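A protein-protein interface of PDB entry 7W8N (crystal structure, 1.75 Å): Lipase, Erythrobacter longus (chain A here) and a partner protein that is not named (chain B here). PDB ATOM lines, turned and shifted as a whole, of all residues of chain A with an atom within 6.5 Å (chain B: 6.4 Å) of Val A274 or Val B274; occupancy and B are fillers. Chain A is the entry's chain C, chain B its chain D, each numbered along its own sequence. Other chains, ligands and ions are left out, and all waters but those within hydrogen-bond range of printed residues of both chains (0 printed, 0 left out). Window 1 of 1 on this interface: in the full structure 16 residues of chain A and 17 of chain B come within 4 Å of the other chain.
The backbone carbonyl oxygen (O) of Val B274 is in hydrogen-bond range of the backbone NH (N) of Tyr A276 (2.8 Å).
N of Tyr B276 lies within hydrogen-bond range of O of Val A274, 2.8 Å away.
O of Leu B267 sits at hydrogen-bond distance from N of Arg B272, at 2.9 Å.
O of Val A275 lies within hydrogen-bond range of N of Val A248 (2.8 Å).
N of Val A275 sits at hydrogen-bond distance from O of Thr A246 (2.9 Å).
The backbone NH (N) of Val B248 lies within hydrogen-bond range of the backbone carbonyl oxygen (O) of Val B275 (2.8 Å).
The backbone NH (N) of Thr A246 lies within hydrogen-bond range of the backbone carbonyl oxygen (O) of Asp A273 (3.3 Å).
The backbone carbonyl oxygen (O) of Val B248 is in hydrogen-bond range of the backbone NH (N) of Leu B277, 2.9 Å away.
Val B268 touches Lys A265 (CG1 to CG, 3.7 Å).
Ala B264 touches Val A268 (CB to CG1, 3.9 Å).
Val A268 touches Lys B265.
Val A268 touches Tyr B276.
Tyr B276 touches Asp A273 (O to CA, 3.3 Å).
Val B274 touches Val A274.
Val A274 touches Val B275.
Val B268 touches Tyr A276 (CG2 to CG, 3.996 Å).
Asp B273 touches Tyr A276 (CA to O, 3.3 Å).
CA of Leu A277 touches OD1 of Asp B273, 3.6 Å away.
Val A274 touches just these residues of chain B: Val B274 (3.8 Å), Val B275 (3.6 Å) and Tyr B276 (2.8 Å).
Val B274 touches just these residues of chain A: Val A274, Val A275 and Tyr A276.
Printed residues of chain A within 4 Å of Leu B277: Asp A273 (3.5 Å).
Printed residues of chain A within 4 Å of Asp B273: Tyr A276 and Leu A277.
Of the printed residues of chain B, Tyr A276 touches Val B268 (3.996 Å), Arg B272 (3.4 Å), Asp B273 (3.3 Å) and Val B274 (2.8 Å).
Of the printed residues of chain B, Arg A272 touches Tyr B276 (3.3 Å).
Pro A245 touches none of the printed residues of chain B.
The nearest residue of chain B that does not touch Val A274 is Leu B277 (5.3 Å).
The nearest residue of chain A that does not touch Val B274 is Leu A277 (5.3 Å).
Of the 16 printed residues of chain A, 8 touch a printed residue of chain B.
Hydrophobic or aromatic side chains of chain A that line the printed part of chain B: Val A268 and Tyr A276.
Hydrophobic or aromatic side chains of chain B within 4 Å of the printed part of chain A: Ala B264, Val B268 and Tyr B276.
Among the printed residues, 17 pairs touch across the chains.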
ATOM      1  N   PRO A 245      -9.705   9.147  31.179  1.00  0.00           N
ATOM      2  CA  PRO A 245      -9.177  10.405  30.615  1.00  0.00           C
ATOM      3  C   PRO A 245      -9.774  10.636  29.236  1.00  0.00           C
ATOM      4  O   PRO A 245      -9.886   9.700  28.448  1.00  0.00           O
ATOM      5  CB  PRO A 245      -7.671  10.154  30.547  1.00  0.00           C
ATOM      6  CG  PRO A 245      -7.415   9.065  31.575  1.00  0.00           C
ATOM      7  CD  PRO A 245      -8.637   8.219  31.586  1.00  0.00           C
ATOM      8  N   THR A 246     -10.199  11.862  28.978  1.00  0.00           N
ATOM      9  CA  THR A 246     -10.985  12.199  27.790  1.00  0.00           C
ATOM     10  C   THR A 246     -10.452  13.421  27.053  1.00  0.00           C
ATOM     11  O   THR A 246     -10.091  14.440  27.660  1.00  0.00           O
ATOM     12  CB  THR A 246     -12.449  12.454  28.197  1.00  0.00           C
ATOM     13  OG1 THR A 246     -12.954  11.284  28.843  1.00  0.00           O
ATOM     14  CG2 THR A 246     -13.345  12.756  26.966  1.00  0.00           C
ATOM     15  N   ILE A 247     -10.498  13.354  25.727  1.00  0.00           N
ATOM     16  CA  ILE A 247     -10.398  14.534  24.867  1.00  0.00           C
ATOM     17  C   ILE A 247     -11.708  14.649  24.096  1.00  0.00           C
ATOM     18  O   ILE A 247     -12.048  13.742  23.333  1.00  0.00           O
ATOM     19  CB  ILE A 247      -9.207  14.428  23.904  1.00  0.00           C
ATOM     20  CG1 ILE A 247      -7.899  14.342  24.680  1.00  0.00           C
ATOM     21  CG2 ILE A 247      -9.197  15.606  22.901  1.00  0.00           C
ATOM     22  CD1 ILE A 247      -6.803  13.723  23.890  1.00  0.00           C
ATOM     23  N   VAL A 248     -12.459  15.719  24.329  1.00  0.00           N
ATOM     24  CA  VAL A 248     -13.647  16.061  23.539  1.00  0.00           C
ATOM     25  C   VAL A 248     -13.263  17.153  22.550  1.00  0.00           C
ATOM     26  O   VAL A 248     -12.869  18.244  22.960  1.00  0.00           O
ATOM     27  CB  VAL A 248     -14.806  16.543  24.428  1.00  0.00           C
ATOM     28  CG1 VAL A 248     -16.049  16.890  23.562  1.00  0.00           C
ATOM     29  CG2 VAL A 248     -15.164  15.504  25.481  1.00  0.00           C
ATOM     30  N   TYR A 263     -21.275  17.140  27.189  1.00  0.00           N
ATOM     31  CA  TYR A 263     -20.543  16.000  27.699  1.00  0.00           C
ATOM     32  C   TYR A 263     -19.299  16.445  28.453  1.00  0.00           C
ATOM     33  O   TYR A 263     -19.000  15.933  29.537  1.00  0.00           O
ATOM     34  CB  TYR A 263     -20.153  15.046  26.578  1.00  0.00           C
ATOM     35  CG  TYR A 263     -19.499  13.799  27.102  1.00  0.00           C
ATOM     36  CD1 TYR A 263     -20.176  12.957  27.980  1.00  0.00           C
ATOM     37  CD2 TYR A 263     -18.201  13.459  26.745  1.00  0.00           C
ATOM     38  CE1 TYR A 263     -19.585  11.827  28.486  1.00  0.00           C
ATOM     39  CE2 TYR A 263     -17.604  12.320  27.242  1.00  0.00           C
ATOM     40  CZ  TYR A 263     -18.291  11.514  28.127  1.00  0.00           C
ATOM     41  OH  TYR A 263     -17.709  10.385  28.632  1.00  0.00           O
ATOM     42  N   ALA A 264     -18.539  17.378  27.889  1.00  0.00           N
ATOM     43  CA  ALA A 264     -17.336  17.807  28.602  1.00  0.00           C
ATOM     44  C   ALA A 264     -17.699  18.476  29.923  1.00  0.00           C
ATOM     45  O   ALA A 264     -17.008  18.276  30.934  1.00  0.00           O
ATOM     46  CB  ALA A 264     -16.503  18.730  27.718  1.00  0.00           C
ATOM     47  N   LYS A 265     -18.798  19.235  29.956  1.00  0.00           N
ATOM     48  CA  LYS A 265     -19.217  19.834  31.225  1.00  0.00           C
ATOM     49  C   LYS A 265     -19.606  18.766  32.247  1.00  0.00           C
ATOM     50  O   LYS A 265     -19.329  18.908  33.445  1.00  0.00           O
ATOM     51  CB  LYS A 265     -20.371  20.797  31.003  1.00  0.00           C
ATOM     52  CG  LYS A 265     -19.992  22.122  30.361  1.00  0.00           C
ATOM     53  CD  LYS A 265     -21.208  22.857  29.894  1.00  0.00           C
ATOM     54  CE  LYS A 265     -21.940  23.485  31.039  1.00  0.00           C
ATOM     55  NZ  LYS A 265     -23.299  23.936  30.622  1.00  0.00           N
ATOM     56  N   LEU A 267     -18.365  15.784  32.467  1.00  0.00           N
ATOM     57  CA  LEU A 267     -17.139  15.185  32.971  1.00  0.00           C
ATOM     58  C   LEU A 267     -16.492  16.077  34.037  1.00  0.00           C
ATOM     59  O   LEU A 267     -16.043  15.571  35.075  1.00  0.00           O
ATOM     60  CB  LEU A 267     -16.163  14.913  31.831  1.00  0.00           C
ATOM     61  CG  LEU A 267     -16.541  13.766  30.887  1.00  0.00           C
ATOM     62  CD1 LEU A 267     -15.462  13.631  29.827  1.00  0.00           C
ATOM     63  CD2 LEU A 267     -16.745  12.457  31.614  1.00  0.00           C
ATOM     64  N   VAL A 268     -16.476  17.390  33.822  1.00  0.00           N
ATOM     65  CA  VAL A 268     -15.930  18.303  34.839  1.00  0.00           C
ATOM     66  C   VAL A 268     -16.769  18.233  36.113  1.00  0.00           C
ATOM     67  O   VAL A 268     -16.238  18.179  37.232  1.00  0.00           O
ATOM     68  CB  VAL A 268     -15.854  19.739  34.303  1.00  0.00           C
ATOM     69  CG1 VAL A 268     -15.382  20.733  35.411  1.00  0.00           C
ATOM     70  CG2 VAL A 268     -14.919  19.832  33.114  1.00  0.00           C
ATOM     71  N   ARG A 272     -13.684  14.566  36.506  1.00  0.00           N
ATOM     72  CA  ARG A 272     -12.878  13.733  35.621  1.00  0.00           C
ATOM     73  C   ARG A 272     -11.958  14.603  34.778  1.00  0.00           C
ATOM     74  O   ARG A 272     -12.316  15.716  34.416  1.00  0.00           O
ATOM     75  CB  ARG A 272     -13.774  12.923  34.678  1.00  0.00           C
ATOM     76  CG  ARG A 272     -14.912  12.201  35.385  1.00  0.00           C
ATOM     77  CD  ARG A 272     -14.410  11.418  36.558  1.00  0.00           C
ATOM     78  NE  ARG A 272     -13.500  10.352  36.163  1.00  0.00           N
ATOM     79  CZ  ARG A 272     -12.601   9.801  36.963  1.00  0.00           C
ATOM     80  NH1 ARG A 272     -12.449  10.248  38.200  1.00  0.00           N
ATOM     81  NH2 ARG A 272     -11.843   8.817  36.518  1.00  0.00           N
ATOM     82  N   ASP A 273     -10.799  14.065  34.411  1.00  0.00           N
ATOM     83  CA  ASP A 273      -9.847  14.842  33.616  1.00  0.00           C
ATOM     84  C   ASP A 273     -10.317  14.890  32.166  1.00  0.00           C
ATOM     85  O   ASP A 273     -10.646  13.846  31.586  1.00  0.00           O
ATOM     86  CB  ASP A 273      -8.459  14.218  33.644  1.00  0.00           C
ATOM     87  CG  ASP A 273      -7.832  14.189  35.035  1.00  0.00           C
ATOM     88  OD1 ASP A 273      -8.268  14.954  35.918  1.00  0.00           O
ATOM     89  OD2 ASP A 273      -6.889  13.385  35.207  1.00  0.00           O
ATOM     90  N   VAL A 274     -10.331  16.082  31.582  1.00  0.00           N
ATOM     91  CA  VAL A 274     -10.831  16.246  30.212  1.00  0.00           C
ATOM     92  C   VAL A 274     -10.158  17.434  29.544  1.00  0.00           C
ATOM     93  O   VAL A 274      -9.995  18.504  30.138  1.00  0.00           O
ATOM     94  CB  VAL A 274     -12.379  16.361  30.182  1.00  0.00           C
ATOM     95  CG1 VAL A 274     -12.904  17.489  31.055  1.00  0.00           C
ATOM     96  CG2 VAL A 274     -12.888  16.529  28.754  1.00  0.00           C
ATOM     97  N   VAL A 275      -9.783  17.232  28.278  1.00  0.00           N
ATOM     98  CA  VAL A 275      -9.349  18.286  27.384  1.00  0.00           C
ATOM     99  C   VAL A 275     -10.525  18.593  26.471  1.00  0.00           C
ATOM    100  O   VAL A 275     -11.047  17.687  25.800  1.00  0.00           O
ATOM    101  CB  VAL A 275      -8.125  17.866  26.552  1.00  0.00           C
ATOM    102  CG1 VAL A 275      -7.719  19.036  25.623  1.00  0.00           C
ATOM    103  CG2 VAL A 275      -6.964  17.415  27.423  1.00  0.00           C
ATOM    104  N   TYR A 276     -10.986  19.830  26.494  1.00  0.00           N
ATOM    105  CA  TYR A 276     -12.056  20.291  25.617  1.00  0.00           C
ATOM    106  C   TYR A 276     -11.476  21.241  24.575  1.00  0.00           C
ATOM    107  O   TYR A 276     -10.957  22.302  24.924  1.00  0.00           O
ATOM    108  CB  TYR A 276     -13.171  20.981  26.409  1.00  0.00           C
ATOM    109  CG  TYR A 276     -14.268  21.425  25.485  1.00  0.00           C
ATOM    110  CD1 TYR A 276     -15.161  20.497  24.946  1.00  0.00           C
ATOM    111  CD2 TYR A 276     -14.379  22.748  25.094  1.00  0.00           C
ATOM    112  CE1 TYR A 276     -16.145  20.891  24.070  1.00  0.00           C
ATOM    113  CE2 TYR A 276     -15.365  23.148  24.185  1.00  0.00           C
ATOM    114  CZ  TYR A 276     -16.242  22.200  23.684  1.00  0.00           C
ATOM    115  OH  TYR A 276     -17.209  22.566  22.782  1.00  0.00           O
ATOM    116  N   LEU A 277     -11.588  20.866  23.294  1.00  0.00           N
ATOM    117  CA  LEU A 277     -11.105  21.678  22.183  1.00  0.00           C
ATOM    118  C   LEU A 277     -12.270  21.948  21.250  1.00  0.00           C
ATOM    119  O   LEU A 277     -12.832  21.003  20.701  1.00  0.00           O
ATOM    120  CB  LEU A 277      -9.998  20.968  21.403  1.00  0.00           C
ATOM    121  CG  LEU A 277      -8.822  20.468  22.237  1.00  0.00           C
ATOM    122  CD1 LEU A 277      -7.893  19.594  21.407  1.00  0.00           C
ATOM    123  CD2 LEU A 277      -8.084  21.615  22.817  1.00  0.00           C
ATOM    124  N   MET A 310      -2.030  13.364  26.885  1.00  0.00           N
ATOM    125  CA  MET A 310      -2.869  12.673  27.842  1.00  0.00           C
ATOM    126  C   MET A 310      -2.459  11.221  28.005  1.00  0.00           C
ATOM    127  O   MET A 310      -2.840  10.602  29.000  1.00  0.00           O
ATOM    128  CB  MET A 310      -4.336  12.754  27.413  1.00  0.00           C
ATOM    129  CG  MET A 310      -5.011  14.098  27.650  1.00  0.00           C
ATOM    130  SD  MET A 310      -5.160  14.679  29.379  1.00  0.00           S
ATOM    131  CE  MET A 310      -6.771  13.949  29.752  1.00  0.00           C
ATOM    132  N   PRO B 245      -6.636  30.331  25.996  1.00  0.00           N
ATOM    133  CA  PRO B 245      -6.453  28.915  26.318  1.00  0.00           C
ATOM    134  C   PRO B 245      -6.162  28.758  27.798  1.00  0.00           C
ATOM    135  O   PRO B 245      -5.383  29.525  28.381  1.00  0.00           O
ATOM    136  CB  PRO B 245      -5.252  28.511  25.462  1.00  0.00           C
ATOM    137  CG  PRO B 245      -5.266  29.504  24.307  1.00  0.00           C
ATOM    138  CD  PRO B 245      -5.713  30.779  24.942  1.00  0.00           C
ATOM    139  N   THR B 246      -6.777  27.748  28.401  1.00  0.00           N
ATOM    140  CA  THR B 246      -6.797  27.618  29.853  1.00  0.00           C
ATOM    141  C   THR B 246      -6.479  26.200  30.297  1.00  0.00           C
ATOM    142  O   THR B 246      -6.953  25.214  29.717  1.00  0.00           O
ATOM    143  CB  THR B 246      -8.158  28.019  30.416  1.00  0.00           C
ATOM    144  OG1 THR B 246      -8.422  29.376  30.111  1.00  0.00           O
ATOM    145  CG2 THR B 246      -8.199  27.831  31.935  1.00  0.00           C
ATOM    146  N   ILE B 247      -5.706  26.092  31.374  1.00  0.00           N
ATOM    147  CA  ILE B 247      -5.552  24.855  32.113  1.00  0.00           C
ATOM    148  C   ILE B 247      -6.042  25.128  33.525  1.00  0.00           C
ATOM    149  O   ILE B 247      -5.495  25.987  34.220  1.00  0.00           O
ATOM    150  CB  ILE B 247      -4.100  24.349  32.141  1.00  0.00           C
ATOM    151  CG1 ILE B 247      -3.624  23.962  30.730  1.00  0.00           C
ATOM    152  CG2 ILE B 247      -3.996  23.160  33.072  1.00  0.00           C
ATOM    153  CD1 ILE B 247      -2.108  24.028  30.580  1.00  0.00           C
ATOM    154  N   VAL B 248      -7.070  24.404  33.952  1.00  0.00           N
ATOM    155  CA  VAL B 248      -7.595  24.504  35.309  1.00  0.00           C
ATOM    156  C   VAL B 248      -7.174  23.240  36.033  1.00  0.00           C
ATOM    157  O   VAL B 248      -7.513  22.127  35.599  1.00  0.00           O
ATOM    158  CB  VAL B 248      -9.133  24.641  35.352  1.00  0.00           C
ATOM    159  CG1 VAL B 248      -9.609  24.650  36.797  1.00  0.00           C
ATOM    160  CG2 VAL B 248      -9.653  25.871  34.637  1.00  0.00           C
ATOM    161  N   TYR B 263     -15.628  27.008  37.098  1.00  0.00           N
ATOM    162  CA  TYR B 263     -14.957  27.838  36.112  1.00  0.00           C
ATOM    163  C   TYR B 263     -14.686  27.057  34.828  1.00  0.00           C
ATOM    164  O   TYR B 263     -14.953  27.550  33.724  1.00  0.00           O
ATOM    165  CB  TYR B 263     -13.657  28.425  36.685  1.00  0.00           C
ATOM    166  CG  TYR B 263     -12.989  29.353  35.700  1.00  0.00           C
ATOM    167  CD1 TYR B 263     -13.636  30.485  35.252  1.00  0.00           C
ATOM    168  CD2 TYR B 263     -11.715  29.087  35.201  1.00  0.00           C
ATOM    169  CE1 TYR B 263     -13.064  31.326  34.330  1.00  0.00           C
ATOM    170  CE2 TYR B 263     -11.121  29.937  34.290  1.00  0.00           C
ATOM    171  CZ  TYR B 263     -11.802  31.056  33.861  1.00  0.00           C
ATOM    172  OH  TYR B 263     -11.274  31.899  32.934  1.00  0.00           O
ATOM    173  N   ALA B 264     -14.178  25.838  34.945  1.00  0.00           N
ATOM    174  CA  ALA B 264     -13.948  25.034  33.744  1.00  0.00           C
ATOM    175  C   ALA B 264     -15.251  24.785  32.981  1.00  0.00           C
ATOM    176  O   ALA B 264     -15.271  24.857  31.751  1.00  0.00           O
ATOM    177  CB  ALA B 264     -13.273  23.723  34.116  1.00  0.00           C
ATOM    178  N   LYS B 265     -16.346  24.505  33.690  1.00  0.00           N
ATOM    179  CA  LYS B 265     -17.639  24.325  33.016  1.00  0.00           C
ATOM    180  C   LYS B 265     -18.077  25.585  32.297  1.00  0.00           C
ATOM    181  O   LYS B 265     -18.630  25.521  31.194  1.00  0.00           O
ATOM    182  CB  LYS B 265     -18.695  23.894  34.033  1.00  0.00           C
ATOM    183  CG  LYS B 265     -18.477  22.502  34.524  1.00  0.00           C
ATOM    184  CD  LYS B 265     -19.360  22.189  35.728  1.00  0.00           C
ATOM    185  CE  LYS B 265     -20.806  22.107  35.309  1.00  0.00           C
ATOM    186  NZ  LYS B 265     -21.702  22.038  36.493  1.00  0.00           N
ATOM    187  N   LEU B 267     -16.106  27.801  30.961  1.00  0.00           N
ATOM    188  CA  LEU B 267     -15.316  27.942  29.742  1.00  0.00           C
ATOM    189  C   LEU B 267     -15.850  27.036  28.635  1.00  0.00           C
ATOM    190  O   LEU B 267     -15.969  27.466  27.486  1.00  0.00           O
ATOM    191  CB  LEU B 267     -13.844  27.635  30.029  1.00  0.00           C
ATOM    192  CG  LEU B 267     -13.140  28.660  30.911  1.00  0.00           C
ATOM    193  CD1 LEU B 267     -11.668  28.317  31.061  1.00  0.00           C
ATOM    194  CD2 LEU B 267     -13.259  30.027  30.331  1.00  0.00           C
ATOM    195  N   VAL B 268     -16.164  25.786  28.958  1.00  0.00           N
ATOM    196  CA  VAL B 268     -16.762  24.887  27.962  1.00  0.00           C
ATOM    197  C   VAL B 268     -18.090  25.455  27.463  1.00  0.00           C
ATOM    198  O   VAL B 268     -18.360  25.483  26.254  1.00  0.00           O
ATOM    199  CB  VAL B 268     -16.945  23.474  28.535  1.00  0.00           C
ATOM    200  CG1 VAL B 268     -17.662  22.567  27.510  1.00  0.00           C
ATOM    201  CG2 VAL B 268     -15.610  22.851  28.968  1.00  0.00           C
ATOM    202  N   ARG B 272     -14.775  27.710  24.858  1.00  0.00           N
ATOM    203  CA  ARG B 272     -13.357  28.005  25.011  1.00  0.00           C
ATOM    204  C   ARG B 272     -12.558  26.722  25.233  1.00  0.00           C
ATOM    205  O   ARG B 272     -13.028  25.786  25.882  1.00  0.00           O
ATOM    206  CB  ARG B 272     -13.144  28.959  26.199  1.00  0.00           C
ATOM    207  CG  ARG B 272     -13.990  30.219  26.175  1.00  0.00           C
ATOM    208  CD  ARG B 272     -14.039  30.884  24.802  1.00  0.00           C
ATOM    209  NE  ARG B 272     -12.741  31.419  24.417  1.00  0.00           N
ATOM    210  CZ  ARG B 272     -12.375  31.642  23.162  1.00  0.00           C
ATOM    211  NH1 ARG B 272     -13.196  31.349  22.152  1.00  0.00           N
ATOM    212  NH2 ARG B 272     -11.174  32.141  22.908  1.00  0.00           N
ATOM    213  N   ASP B 273     -11.331  26.688  24.712  1.00  0.00           N
ATOM    214  CA  ASP B 273     -10.473  25.523  24.914  1.00  0.00           C
ATOM    215  C   ASP B 273      -9.957  25.495  26.351  1.00  0.00           C
ATOM    216  O   ASP B 273      -9.411  26.489  26.847  1.00  0.00           O
ATOM    217  CB  ASP B 273      -9.262  25.521  23.972  1.00  0.00           C
ATOM    218  CG  ASP B 273      -9.635  25.568  22.496  1.00  0.00           C
ATOM    219  OD1 ASP B 273     -10.774  25.219  22.141  1.00  0.00           O
ATOM    220  OD2 ASP B 273      -8.759  25.974  21.695  1.00  0.00           O
ATOM    221  N   VAL B 274     -10.071  24.340  26.986  1.00  0.00           N
ATOM    222  CA  VAL B 274      -9.672  24.204  28.381  1.00  0.00           C
ATOM    223  C   VAL B 274      -9.250  22.771  28.673  1.00  0.00           C
ATOM    224  O   VAL B 274      -9.858  21.801  28.208  1.00  0.00           O
ATOM    225  CB  VAL B 274     -10.792  24.691  29.327  1.00  0.00           C
ATOM    226  CG1 VAL B 274     -12.110  24.063  28.982  1.00  0.00           C
ATOM    227  CG2 VAL B 274     -10.403  24.408  30.783  1.00  0.00           C
ATOM    228  N   VAL B 275      -8.167  22.636  29.440  1.00  0.00           N
ATOM    229  CA  VAL B 275      -7.748  21.375  30.034  1.00  0.00           C
ATOM    230  C   VAL B 275      -8.182  21.420  31.498  1.00  0.00           C
ATOM    231  O   VAL B 275      -7.795  22.342  32.233  1.00  0.00           O
ATOM    232  CB  VAL B 275      -6.226  21.159  29.919  1.00  0.00           C
ATOM    233  CG1 VAL B 275      -5.825  19.848  30.571  1.00  0.00           C
ATOM    234  CG2 VAL B 275      -5.755  21.220  28.461  1.00  0.00           C
ATOM    235  N   TYR B 276      -9.013  20.461  31.912  1.00  0.00           N
ATOM    236  CA  TYR B 276      -9.444  20.335  33.300  1.00  0.00           C
ATOM    237  C   TYR B 276      -8.757  19.115  33.909  1.00  0.00           C
ATOM    238  O   TYR B 276      -8.933  17.991  33.430  1.00  0.00           O
ATOM    239  CB  TYR B 276     -10.977  20.218  33.412  1.00  0.00           C
ATOM    240  CG  TYR B 276     -11.368  20.084  34.865  1.00  0.00           C
ATOM    241  CD1 TYR B 276     -11.299  21.183  35.699  1.00  0.00           C
ATOM    242  CD2 TYR B 276     -11.729  18.850  35.418  1.00  0.00           C
ATOM    243  CE1 TYR B 276     -11.603  21.097  37.018  1.00  0.00           C
ATOM    244  CE2 TYR B 276     -12.037  18.750  36.776  1.00  0.00           C
ATOM    245  CZ  TYR B 276     -11.951  19.907  37.568  1.00  0.00           C
ATOM    246  OH  TYR B 276     -12.214  19.907  38.928  1.00  0.00           O
ATOM    247  N   LEU B 277      -7.941  19.338  34.950  1.00  0.00           N
ATOM    248  CA  LEU B 277      -7.216  18.291  35.655  1.00  0.00           C
ATOM    249  C   LEU B 277      -7.608  18.370  37.127  1.00  0.00           C
ATOM    250  O   LEU B 277      -7.408  19.405  37.768  1.00  0.00           O
ATOM    251  CB  LEU B 277      -5.695  18.445  35.507  1.00  0.00           C
ATOM    252  CG  LEU B 277      -5.124  18.455  34.089  1.00  0.00           C
ATOM    253  CD1 LEU B 277      -3.622  18.680  34.138  1.00  0.00           C
ATOM    254  CD2 LEU B 277      -5.464  17.156  33.328  1.00  0.00           C
ATOM    255  N   MET B 310      -0.321  22.935  25.373  1.00  0.00           N
ATOM    256  CA  MET B 310      -1.224  24.026  25.042  1.00  0.00           C
ATOM    257  C   MET B 310      -0.490  25.221  24.465  1.00  0.00           C
ATOM    258  O   MET B 310      -1.121  26.023  23.768  1.00  0.00           O
ATOM    259  CB  MET B 310      -2.053  24.441  26.268  1.00  0.00           C
ATOM    260  CG  MET B 310      -3.048  23.350  26.733  1.00  0.00           C
ATOM    261  SD  MET B 310      -4.358  23.008  25.535  1.00  0.00           S
ATOM    262  CE  MET B 310      -5.474  24.326  25.880  1.00  0.00           C
